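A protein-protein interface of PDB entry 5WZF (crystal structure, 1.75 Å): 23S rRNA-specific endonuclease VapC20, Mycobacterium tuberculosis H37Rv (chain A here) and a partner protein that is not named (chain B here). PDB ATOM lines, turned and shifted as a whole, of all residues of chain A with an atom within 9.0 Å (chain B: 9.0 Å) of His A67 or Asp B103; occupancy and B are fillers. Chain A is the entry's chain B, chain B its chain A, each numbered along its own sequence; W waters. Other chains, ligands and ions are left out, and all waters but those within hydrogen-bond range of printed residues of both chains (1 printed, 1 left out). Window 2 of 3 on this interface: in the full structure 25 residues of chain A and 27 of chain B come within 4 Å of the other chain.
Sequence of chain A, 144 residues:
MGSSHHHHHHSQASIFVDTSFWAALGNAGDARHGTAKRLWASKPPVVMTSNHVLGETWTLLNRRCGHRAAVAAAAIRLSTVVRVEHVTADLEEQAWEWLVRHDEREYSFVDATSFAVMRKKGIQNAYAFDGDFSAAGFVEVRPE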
ATOM      1  N   TRP A  58     -25.992  22.500   5.626  1.00  0.00           N
ATOM      2  CA  TRP A  58     -25.598  21.799   6.847  1.00  0.00           C
ATOM      3  C   TRP A  58     -26.824  21.372   7.644  1.00  0.00           C
ATOM      4  O   TRP A  58     -26.973  20.207   8.017  1.00  0.00           O
ATOM      5  CB  TRP A  58     -24.705  22.674   7.738  1.00  0.00           C
ATOM      6  CG  TRP A  58     -24.599  22.131   9.142  1.00  0.00           C
ATOM      7  CD1 TRP A  58     -25.458  22.365  10.179  1.00  0.00           C
ATOM      8  CD2 TRP A  58     -23.599  21.239   9.645  1.00  0.00           C
ATOM      9  NE1 TRP A  58     -25.053  21.676  11.297  1.00  0.00           N
ATOM     10  CE2 TRP A  58     -23.913  20.978  10.996  1.00  0.00           C
ATOM     11  CE3 TRP A  58     -22.464  20.642   9.089  1.00  0.00           C
ATOM     12  CZ2 TRP A  58     -23.131  20.147  11.799  1.00  0.00           C
ATOM     13  CZ3 TRP A  58     -21.689  19.811   9.890  1.00  0.00           C
ATOM     14  CH2 TRP A  58     -22.028  19.575  11.228  1.00  0.00           C
ATOM     15  N   THR A  59     -27.696  22.335   7.908  1.00  0.00           N
ATOM     16  CA  THR A  59     -28.829  22.115   8.790  1.00  0.00           C
ATOM     17  C   THR A  59     -29.754  21.048   8.230  1.00  0.00           C
ATOM     18  O   THR A  59     -30.199  20.160   8.954  1.00  0.00           O
ATOM     19  CB  THR A  59     -29.597  23.423   9.021  1.00  0.00           C
ATOM     20  OG1 THR A  59     -28.725  24.368   9.657  1.00  0.00           O
ATOM     21  CG2 THR A  59     -30.819  23.185   9.906  1.00  0.00           C
ATOM     22  N   LEU A  60     -30.011  21.123   6.929  1.00  0.00           N
ATOM     23  CA  LEU A  60     -30.881  20.167   6.257  1.00  0.00           C
ATOM     24  C   LEU A  60     -30.297  18.751   6.269  1.00  0.00           C
ATOM     25  O   LEU A  60     -30.989  17.790   6.609  1.00  0.00           O
ATOM     26  CB  LEU A  60     -31.142  20.628   4.821  1.00  0.00           C
ATOM     27  CG  LEU A  60     -32.212  19.891   4.017  1.00  0.00           C
ATOM     28  CD1 LEU A  60     -33.524  19.860   4.774  1.00  0.00           C
ATOM     29  CD2 LEU A  60     -32.394  20.559   2.665  1.00  0.00           C
ATOM     30  N   LEU A  61     -29.022  18.628   5.906  1.00  0.00           N
ATOM     31  CA  LEU A  61     -28.356  17.326   5.874  1.00  0.00           C
ATOM     32  C   LEU A  61     -28.172  16.733   7.274  1.00  0.00           C
ATOM     33  O   LEU A  61     -28.277  15.518   7.461  1.00  0.00           O
ATOM     34  CB  LEU A  61     -27.000  17.441   5.172  1.00  0.00           C
ATOM     35  CG  LEU A  61     -27.051  17.625   3.650  1.00  0.00           C
ATOM     36  CD1 LEU A  61     -25.647  17.702   3.063  1.00  0.00           C
ATOM     37  CD2 LEU A  61     -27.833  16.493   3.014  1.00  0.00           C
ATOM     38  N   ASN A  62     -27.900  17.590   8.253  1.00  0.00           N
ATOM     39  CA  ASN A  62     -27.727  17.137   9.630  1.00  0.00           C
ATOM     40  C   ASN A  62     -29.041  16.574  10.162  1.00  0.00           C
ATOM     41  O   ASN A  62     -29.059  15.596  10.912  1.00  0.00           O
ATOM     42  CB  ASN A  62     -27.227  18.284  10.517  1.00  0.00           C
ATOM     43  CG  ASN A  62     -26.615  17.796  11.817  1.00  0.00           C
ATOM     44  OD1 ASN A  62     -26.152  16.662  11.906  1.00  0.00           O
ATOM     45  ND2 ASN A  62     -26.613  18.651  12.830  1.00  0.00           N
ATOM     46  N   ARG A  63     -30.143  17.189   9.747  1.00  0.00           N
ATOM     47  CA  ARG A  63     -31.471  16.754  10.164  1.00  0.00           C
ATOM     48  C   ARG A  63     -31.911  15.476   9.460  1.00  0.00           C
ATOM     49  O   ARG A  63     -32.411  14.550  10.096  1.00  0.00           O
ATOM     50  CB  ARG A  63     -32.500  17.861   9.911  1.00  0.00           C
ATOM     51  CG  ARG A  63     -32.422  19.007  10.903  1.00  0.00           C
ATOM     52  CD  ARG A  63     -33.373  20.144  10.557  1.00  0.00           C
ATOM     53  NE  ARG A  63     -33.359  21.177  11.593  1.00  0.00           N
ATOM     54  CZ  ARG A  63     -33.810  22.416  11.428  1.00  0.00           C
ATOM     55  NH1 ARG A  63     -34.308  22.792  10.258  1.00  0.00           N
ATOM     56  NH2 ARG A  63     -33.752  23.282  12.432  1.00  0.00           N
ATOM     57  N   ARG A  64     -31.712  15.428   8.147  1.00  0.00           N
ATOM     58  CA  ARG A  64     -32.187  14.309   7.342  1.00  0.00           C
ATOM     59  C   ARG A  64     -31.286  13.080   7.440  1.00  0.00           C
ATOM     60  O   ARG A  64     -31.773  11.954   7.528  1.00  0.00           O
ATOM     61  CB  ARG A  64     -32.326  14.728   5.875  1.00  0.00           C
ATOM     62  CG  ARG A  64     -33.710  14.476   5.304  1.00  0.00           C
ATOM     63  CD  ARG A  64     -33.696  14.385   3.789  1.00  0.00           C
ATOM     64  NE  ARG A  64     -34.449  13.224   3.324  1.00  0.00           N
ATOM     65  CZ  ARG A  64     -34.922  13.078   2.091  1.00  0.00           C
ATOM     66  NH1 ARG A  64     -34.725  14.027   1.186  1.00  0.00           N
ATOM     67  NH2 ARG A  64     -35.595  11.985   1.763  1.00  0.00           N
ATOM     68  N   CSO A  65     -29.976  13.297   7.419  1.00  0.00           N
ATOM     69  CA  CSO A  65     -29.024  12.189   7.462  1.00  0.00           C
ATOM     70  CB  CSO A  65     -28.037  12.267   6.297  1.00  0.00           C
ATOM     71  SG  CSO A  65     -28.949  12.317   4.741  1.00  0.00           S
ATOM     72  C   CSO A  65     -28.282  12.030   8.782  1.00  0.00           C
ATOM     73  O   CSO A  65     -27.441  11.137   8.916  1.00  0.00           O
ATOM     74  OD  CSO A  65     -29.297  10.650   4.214  1.00  0.00           O
ATOM     75  N   GLY A  66     -27.716  13.121   9.280  1.00  0.00           N
ATOM     76  CA  GLY A  66     -26.938  13.066  10.499  1.00  0.00           C
ATOM     77  C   GLY A  66     -25.631  13.811  10.351  1.00  0.00           C
ATOM     78  O   GLY A  66     -25.363  14.410   9.311  1.00  0.00           O
ATOM     79  N   HIS A  67     -24.811  13.751  11.394  1.00  0.00           N
ATOM     80  CA  HIS A  67     -23.626  14.593  11.502  1.00  0.00           C
ATOM     81  C   HIS A  67     -22.584  14.341  10.410  1.00  0.00           C
ATOM     82  O   HIS A  67     -21.999  15.286   9.882  1.00  0.00           O
ATOM     83  CB  HIS A  67     -22.989  14.401  12.881  1.00  0.00           C
ATOM     84  CG  HIS A  67     -21.898  15.379  13.181  1.00  0.00           C
ATOM     85  ND1 HIS A  67     -20.565  15.085  12.999  1.00  0.00           N
ATOM     86  CD2 HIS A  67     -21.945  16.653  13.637  1.00  0.00           C
ATOM     87  CE1 HIS A  67     -19.837  16.134  13.336  1.00  0.00           C
ATOM     88  NE2 HIS A  67     -20.649  17.099  13.726  1.00  0.00           N
ATOM     89  N   ARG A  68     -22.360  13.076  10.066  1.00  0.00           N
ATOM     90  CA  ARG A  68     -21.323  12.728   9.097  1.00  0.00           C
ATOM     91  C   ARG A  68     -21.620  13.301   7.711  1.00  0.00           C
ATOM     92  O   ARG A  68     -20.748  13.891   7.075  1.00  0.00           O
ATOM     93  CB  ARG A  68     -21.157  11.208   9.011  1.00  0.00           C
ATOM     94  CG  ARG A  68     -19.959  10.764   8.186  1.00  0.00           C
ATOM     95  CD  ARG A  68     -19.800   9.251   8.217  1.00  0.00           C
ATOM     96  NE  ARG A  68     -18.590   8.806   7.534  1.00  0.00           N
ATOM     97  CZ  ARG A  68     -18.537   8.480   6.247  1.00  0.00           C
ATOM     98  NH1 ARG A  68     -19.630   8.556   5.500  1.00  0.00           N
ATOM     99  NH2 ARG A  68     -17.391   8.080   5.705  1.00  0.00           N
ATOM    100  N   ALA A  69     -22.851  13.125   7.245  1.00  0.00           N
ATOM    101  CA  ALA A  69     -23.250  13.661   5.951  1.00  0.00           C
ATOM    102  C   ALA A  69     -23.144  15.184   5.938  1.00  0.00           C
ATOM    103  O   ALA A  69     -22.750  15.785   4.936  1.00  0.00           O
ATOM    104  CB  ALA A  69     -24.661  13.222   5.610  1.00  0.00           C
ATOM    105  N   ALA A  70     -23.492  15.799   7.063  1.00  0.00           N
ATOM    106  CA  ALA A  70     -23.463  17.250   7.190  1.00  0.00           C
ATOM    107  C   ALA A  70     -22.027  17.769   7.133  1.00  0.00           C
ATOM    108  O   ALA A  70     -21.761  18.825   6.563  1.00  0.00           O
ATOM    109  CB  ALA A  70     -24.143  17.681   8.486  1.00  0.00           C
ATOM    110  N   VAL A  71     -21.098  17.009   7.704  1.00  0.00           N
ATOM    111  CA  VAL A  71     -19.691  17.397   7.707  1.00  0.00           C
ATOM    112  C   VAL A  71     -19.158  17.510   6.275  1.00  0.00           C
ATOM    113  O   VAL A  71     -18.325  18.368   5.971  1.00  0.00           O
ATOM    114  CB  VAL A  71     -18.851  16.400   8.533  1.00  0.00           C
ATOM    115  CG1 VAL A  71     -17.372  16.554   8.247  1.00  0.00           C
ATOM    116  CG2 VAL A  71     -19.127  16.597  10.016  1.00  0.00           C
ATOM    117  N   ALA A  72     -19.676  16.667   5.389  1.00  0.00           N
ATOM    118  CA  ALA A  72     -19.310  16.731   3.979  1.00  0.00           C
ATOM    119  C   ALA A  72     -19.655  18.094   3.380  1.00  0.00           C
ATOM    120  O   ALA A  72     -18.886  18.653   2.599  1.00  0.00           O
ATOM    121  CB  ALA A  72     -19.998  15.624   3.204  1.00  0.00           C
ATOM    122  N   ALA A  73     -20.812  18.630   3.760  1.00  0.00           N
ATOM    123  CA  ALA A  73     -21.251  19.932   3.270  1.00  0.00           C
ATOM    124  C   ALA A  73     -20.403  21.056   3.855  1.00  0.00           C
ATOM    125  O   ALA A  73     -20.112  22.044   3.179  1.00  0.00           O
ATOM    126  CB  ALA A  73     -22.721  20.152   3.597  1.00  0.00           C
ATOM    127  N   ALA A  74     -20.014  20.899   5.116  1.00  0.00           N
ATOM    128  CA  ALA A  74     -19.162  21.874   5.787  1.00  0.00           C
ATOM    129  C   ALA A  74     -17.839  22.042   5.041  1.00  0.00           C
ATOM    130  O   ALA A  74     -17.285  23.138   4.971  1.00  0.00           O
ATOM    131  CB  ALA A  74     -18.908  21.451   7.228  1.00  0.00           C
ATOM    132  N   ALA B  95     -17.807  28.822  13.968  1.00  0.00           N
ATOM    133  CA  ALA B  95     -19.045  28.056  14.066  1.00  0.00           C
ATOM    134  C   ALA B  95     -18.942  26.728  13.311  1.00  0.00           C
ATOM    135  O   ALA B  95     -19.394  25.695  13.797  1.00  0.00           O
ATOM    136  CB  ALA B  95     -20.215  28.875  13.547  1.00  0.00           C
ATOM    137  N   TRP B  96     -18.343  26.762  12.126  1.00  0.00           N
ATOM    138  CA  TRP B  96     -18.130  25.545  11.347  1.00  0.00           C
ATOM    139  C   TRP B  96     -17.257  24.536  12.097  1.00  0.00           C
ATOM    140  O   TRP B  96     -17.588  23.353  12.183  1.00  0.00           O
ATOM    141  CB  TRP B  96     -17.483  25.873  10.005  1.00  0.00           C
ATOM    142  CG  TRP B  96     -18.420  26.417   8.964  1.00  0.00           C
ATOM    143  CD1 TRP B  96     -18.338  27.629   8.341  1.00  0.00           C
ATOM    144  CD2 TRP B  96     -19.562  25.755   8.406  1.00  0.00           C
ATOM    145  NE1 TRP B  96     -19.363  27.762   7.431  1.00  0.00           N
ATOM    146  CE2 TRP B  96     -20.128  26.627   7.454  1.00  0.00           C
ATOM    147  CE3 TRP B  96     -20.166  24.512   8.626  1.00  0.00           C
ATOM    148  CZ2 TRP B  96     -21.267  26.296   6.720  1.00  0.00           C
ATOM    149  CZ3 TRP B  96     -21.300  24.186   7.899  1.00  0.00           C
ATOM    150  CH2 TRP B  96     -21.837  25.074   6.956  1.00  0.00           C
ATOM    151  N   GLU B  97     -16.138  25.014  12.628  1.00  0.00           N
ATOM    152  CA  GLU B  97     -15.226  24.143  13.353  1.00  0.00           C
ATOM    153  C   GLU B  97     -15.924  23.579  14.590  1.00  0.00           C
ATOM    154  O   GLU B  97     -15.762  22.409  14.917  1.00  0.00           O
ATOM    155  CB  GLU B  97     -13.947  24.894  13.725  1.00  0.00           C
ATOM    156  CG  GLU B  97     -13.154  25.356  12.507  1.00  0.00           C
ATOM    157  CD  GLU B  97     -11.850  26.046  12.865  1.00  0.00           C
ATOM    158  OE1 GLU B  97     -11.574  26.223  14.069  1.00  0.00           O
ATOM    159  OE2 GLU B  97     -11.100  26.413  11.935  1.00  0.00           O
ATOM    160  N   TRP B  98     -16.731  24.412  15.240  1.00  0.00           N
ATOM    161  CA  TRP B  98     -17.546  23.987  16.373  1.00  0.00           C
ATOM    162  C   TRP B  98     -18.544  22.884  15.984  1.00  0.00           C
ATOM    163  O   TRP B  98     -18.662  21.872  16.676  1.00  0.00           O
ATOM    164  CB  TRP B  98     -18.294  25.193  16.962  1.00  0.00           C
ATOM    165  CG  TRP B  98     -18.976  24.909  18.268  1.00  0.00           C
ATOM    166  CD1 TRP B  98     -18.444  25.048  19.518  1.00  0.00           C
ATOM    167  CD2 TRP B  98     -20.315  24.435  18.452  1.00  0.00           C
ATOM    168  NE1 TRP B  98     -19.371  24.691  20.469  1.00  0.00           N
ATOM    169  CE2 TRP B  98     -20.527  24.311  19.839  1.00  0.00           C
ATOM    170  CE3 TRP B  98     -21.355  24.102  17.577  1.00  0.00           C
ATOM    171  CZ2 TRP B  98     -21.737  23.867  20.372  1.00  0.00           C
ATOM    172  CZ3 TRP B  98     -22.553  23.663  18.109  1.00  0.00           C
ATOM    173  CH2 TRP B  98     -22.734  23.548  19.493  1.00  0.00           C
ATOM    174  N   LEU B  99     -19.255  23.089  14.876  1.00  0.00           N
ATOM    175  CA  LEU B  99     -20.234  22.116  14.385  1.00  0.00           C
ATOM    176  C   LEU B  99     -19.610  20.762  14.097  1.00  0.00           C
ATOM    177  O   LEU B  99     -20.184  19.719  14.412  1.00  0.00           O
ATOM    178  CB  LEU B  99     -20.913  22.630  13.117  1.00  0.00           C
ATOM    179  CG  LEU B  99     -21.978  23.706  13.303  1.00  0.00           C
ATOM    180  CD1 LEU B  99     -22.334  24.335  11.962  1.00  0.00           C
ATOM    181  CD2 LEU B  99     -23.209  23.117  13.977  1.00  0.00           C
ATOM    182  N   VAL B 100     -18.433  20.785  13.490  1.00  0.00           N
ATOM    183  CA  VAL B 100     -17.749  19.552  13.136  1.00  0.00           C
ATOM    184  C   VAL B 100     -17.367  18.760  14.389  1.00  0.00           C
ATOM    185  O   VAL B 100     -17.438  17.533  14.395  1.00  0.00           O
ATOM    186  CB  VAL B 100     -16.497  19.842  12.279  1.00  0.00           C
ATOM    187  CG1 VAL B 100     -15.680  18.573  12.047  1.00  0.00           C
ATOM    188  CG2 VAL B 100     -16.909  20.469  10.953  1.00  0.00           C
ATOM    189  N   ARG B 101     -16.978  19.468  15.447  1.00  0.00           N
ATOM    190  CA  ARG B 101     -16.564  18.820  16.689  1.00  0.00           C
ATOM    191  C   ARG B 101     -17.744  18.241  17.460  1.00  0.00           C
ATOM    192  O   ARG B 101     -17.667  17.133  17.988  1.00  0.00           O
ATOM    193  CB  ARG B 101     -15.808  19.798  17.596  1.00  0.00           C
ATOM    194  CG  ARG B 101     -14.475  20.285  17.053  1.00  0.00           C
ATOM    195  CD  ARG B 101     -13.619  20.884  18.163  1.00  0.00           C
ATOM    196  NE  ARG B 101     -14.405  21.671  19.110  1.00  0.00           N
ATOM    197  CZ  ARG B 101     -14.701  22.957  18.951  1.00  0.00           C
ATOM    198  NH1 ARG B 101     -15.419  23.592  19.868  1.00  0.00           N
ATOM    199  NH2 ARG B 101     -14.280  23.609  17.876  1.00  0.00           N
ATOM    200  N   HIS B 102     -18.832  18.998  17.531  1.00  0.00           N
ATOM    201  CA  HIS B 102     -19.958  18.628  18.382  1.00  0.00           C
ATOM    202  C   HIS B 102     -20.966  17.702  17.706  1.00  0.00           C
ATOM    203  O   HIS B 102     -22.041  18.132  17.288  1.00  0.00           O
ATOM    204  CB  HIS B 102     -20.652  19.889  18.889  1.00  0.00           C
ATOM    205  CG  HIS B 102     -19.856  20.629  19.918  1.00  0.00           C
ATOM    206  ND1 HIS B 102     -20.110  20.529  21.269  1.00  0.00           N
ATOM    207  CD2 HIS B 102     -18.793  21.458  19.795  1.00  0.00           C
ATOM    208  CE1 HIS B 102     -19.248  21.278  21.932  1.00  0.00           C
ATOM    209  NE2 HIS B 102     -18.436  21.850  21.062  1.00  0.00           N
ATOM    210  N   ASP B 103     -20.613  16.422  17.638  1.00  0.00           N
ATOM    211  CA  ASP B 103     -21.464  15.408  17.026  1.00  0.00           C
ATOM    212  C   ASP B 103     -22.402  14.756  18.038  1.00  0.00           C
ATOM    213  O   ASP B 103     -23.181  13.870  17.689  1.00  0.00           O
ATOM    214  CB  ASP B 103     -20.606  14.331  16.358  1.00  0.00           C
ATOM    215  CG  ASP B 103     -19.751  13.566  17.352  1.00  0.00           C
ATOM    216  OD1 ASP B 103     -19.301  14.174  18.347  1.00  0.00           O
ATOM    217  OD2 ASP B 103     -19.530  12.355  17.142  1.00  0.00           O
ATOM    218  N   GLU B 104     -22.323  15.190  19.293  1.00  0.00           N
ATOM    219  CA  GLU B 104     -23.096  14.557  20.360  1.00  0.00           C
ATOM    220  C   GLU B 104     -24.562  14.975  20.326  1.00  0.00           C
ATOM    221  O   GLU B 104     -25.402  14.376  20.995  1.00  0.00           O
ATOM    222  CB  GLU B 104     -22.500  14.892  21.731  1.00  0.00           C
ATOM    223  CG  GLU B 104     -22.792  16.307  22.216  1.00  0.00           C
ATOM    224  CD  GLU B 104     -21.840  17.339  21.642  1.00  0.00           C
ATOM    225  OE1 GLU B 104     -20.847  16.943  21.000  1.00  0.00           O
ATOM    226  OE2 GLU B 104     -22.085  18.546  21.837  1.00  0.00           O
ATOM    227  N   ARG B 105     -24.864  16.003  19.542  1.00  0.00           N
ATOM    228  CA  ARG B 105     -26.209  16.561  19.502  1.00  0.00           C
ATOM    229  C   ARG B 105     -26.460  17.227  18.152  1.00  0.00           C
ATOM    230  O   ARG B 105     -25.523  17.667  17.489  1.00  0.00           O
ATOM    231  CB  ARG B 105     -26.393  17.558  20.652  1.00  0.00           C
ATOM    232  CG  ARG B 105     -27.823  18.001  20.923  1.00  0.00           C
ATOM    233  CD  ARG B 105     -27.878  18.864  22.180  1.00  0.00           C
ATOM    234  NE  ARG B 105     -29.142  19.582  22.315  1.00  0.00           N
ATOM    235  CZ  ARG B 105     -30.104  19.259  23.173  1.00  0.00           C
ATOM    236  NH1 ARG B 105     -31.217  19.980  23.216  1.00  0.00           N
ATOM    237  NH2 ARG B 105     -29.952  18.225  23.991  1.00  0.00           N
ATOM    238  N   GLU B 106     -27.722  17.289  17.740  1.00  0.00           N
ATOM    239  CA  GLU B 106     -28.071  17.895  16.461  1.00  0.00           C
ATOM    240  C   GLU B 106     -28.170  19.414  16.576  1.00  0.00           C
ATOM    241  O   GLU B 106     -29.114  19.943  17.165  1.00  0.00           O
ATOM    242  CB  GLU B 106     -29.387  17.320  15.937  1.00  0.00           C
ATOM    243  CG  GLU B 106     -29.841  17.926  14.621  1.00  0.00           C
ATOM    244  CD  GLU B 106     -31.246  17.512  14.244  1.00  0.00           C
ATOM    245  OE1 GLU B 106     -31.543  16.299  14.282  1.00  0.00           O
ATOM    246  OE2 GLU B 106     -32.058  18.402  13.921  1.00  0.00           O
ATOM    247  N   TYR B 107     -27.184  20.107  16.012  1.00  0.00           N
ATOM    248  CA  TYR B 107     -27.135  21.566  16.050  1.00  0.00           C
ATOM    249  C   TYR B 107     -27.280  22.169  14.657  1.00  0.00           C
ATOM    250  O   TYR B 107     -26.691  21.675  13.698  1.00  0.00           O
ATOM    251  CB  TYR B 107     -25.822  22.051  16.666  1.00  0.00           C
ATOM    252  CG  TYR B 107     -25.705  21.858  18.164  1.00  0.00           C
ATOM    253  CD1 TYR B 107     -26.427  22.652  19.046  1.00  0.00           C
ATOM    254  CD2 TYR B 107     -24.848  20.901  18.695  1.00  0.00           C
ATOM    255  CE1 TYR B 107     -26.315  22.487  20.419  1.00  0.00           C
ATOM    256  CE2 TYR B 107     -24.728  20.727  20.065  1.00  0.00           C
ATOM    257  CZ  TYR B 107     -25.463  21.521  20.922  1.00  0.00           C
ATOM    258  OH  TYR B 107     -25.344  21.354  22.284  1.00  0.00           O
HETATM  259  O   HOH W   1     -25.023  18.459  15.147  1.00  0.00           O
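NE2 of His B102 is in hydrogen-bond range of NE1 of Trp B98, at 3.0 Å.
N of His A67 lies within hydrogen-bond range of OD1 of Asn A62 (3.2 Å).
OE2 of Glu B104 sits at hydrogen-bond distance from ND1 of His B102, 2.9 Å away.
Water W1 lies within hydrogen-bond range of the backbone carbonyl oxygen (O) of Arg B105 (2.5 Å), the side-chain amide nitrogen (ND2) of Asn A62 (2.8 Å) and the backbone NH (N) of Tyr B107 (2.9 Å).
Among the printed residues, pairs that only touch across the chains: His A67 with Asp B103 (3.4 Å), Trp A58 with Leu B99 (3.6 Å), Ala A74 with Trp B96 (3.6 Å), Trp A58 with Trp B96 (3.7 Å), Asn A62 with Glu B106 (3.8 Å) and His A67 with His B102 (3.9 Å).
Of chain B, only Leu B99 (2.7 Å), Val B100 (3.0 Å), His B102 (3.9 Å) and Asp B103 (3.4 Å) come within 4 Å of His A67.
Asp B103 touches just one residue of chain A: His A67.
No residue of chain B comes within 4 Å of Ala A70.
No residue of chain A comes within 4 Å of Glu B104.
Of the printed residues of chain B, Trp A58 touches Trp B96, Leu B99 and Tyr B107.
Of the printed residues of chain A, Val B100 touches His A67 (3.0 Å).
Of the printed residues of chain B, Asn A62 touches Glu B106 and Tyr B107.
Arg A64 touches none of the printed residues of chain B.
Thr A59 touches none of the printed residues of chain B.
The nearest printed residue of chain B that does not touch His A67 is Arg B101 (4.7 Å).
The nearest printed residue of chain B that does not touch Arg A63 is Tyr B107 (6.9 Å).
The backbone carbonyl oxygen (O) of Tyr B107 is in hydrogen-bond range of the side-chain amide nitrogen (ND2) of Asn A62, at 3.1 Å.
The indole nitrogen (NE1) of Trp A58 lies within hydrogen-bond range of the backbone carbonyl oxygen (O) of Tyr B107 (2.9 Å).
The side-chain carboxylate of Glu B106 lies within salt-bridge range of the guanidinium group of Arg A63, 3.8 Å away.
A ring nitrogen (NE2) of His A67 lies within hydrogen-bond range of the backbone carbonyl oxygen (O) of Leu B99 (2.7 Å).
A ring nitrogen (NE2) of His A67 sits close to the backbone carbonyl oxygen of Val B100 (3.3 Å).
Hydrophobic or aromatic side chains of chain A within 4 Å of the printed part of chain B: Trp A58, His A67 and Ala A74.
Along chain A the printed residues that touch a printed residue of chain B span positions 58 to 74.
Along chain B the printed residues that touch a printed residue of chain A span positions 96 to 107.
Among the printed residues, 11 pairs touch across the chains.
Among the printed residues, Asp or Glu carboxylates within 4 Å of a Lys or Arg side-chain nitrogen of the other chain: Arg A63 with Glu B106 (3.8 Å).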
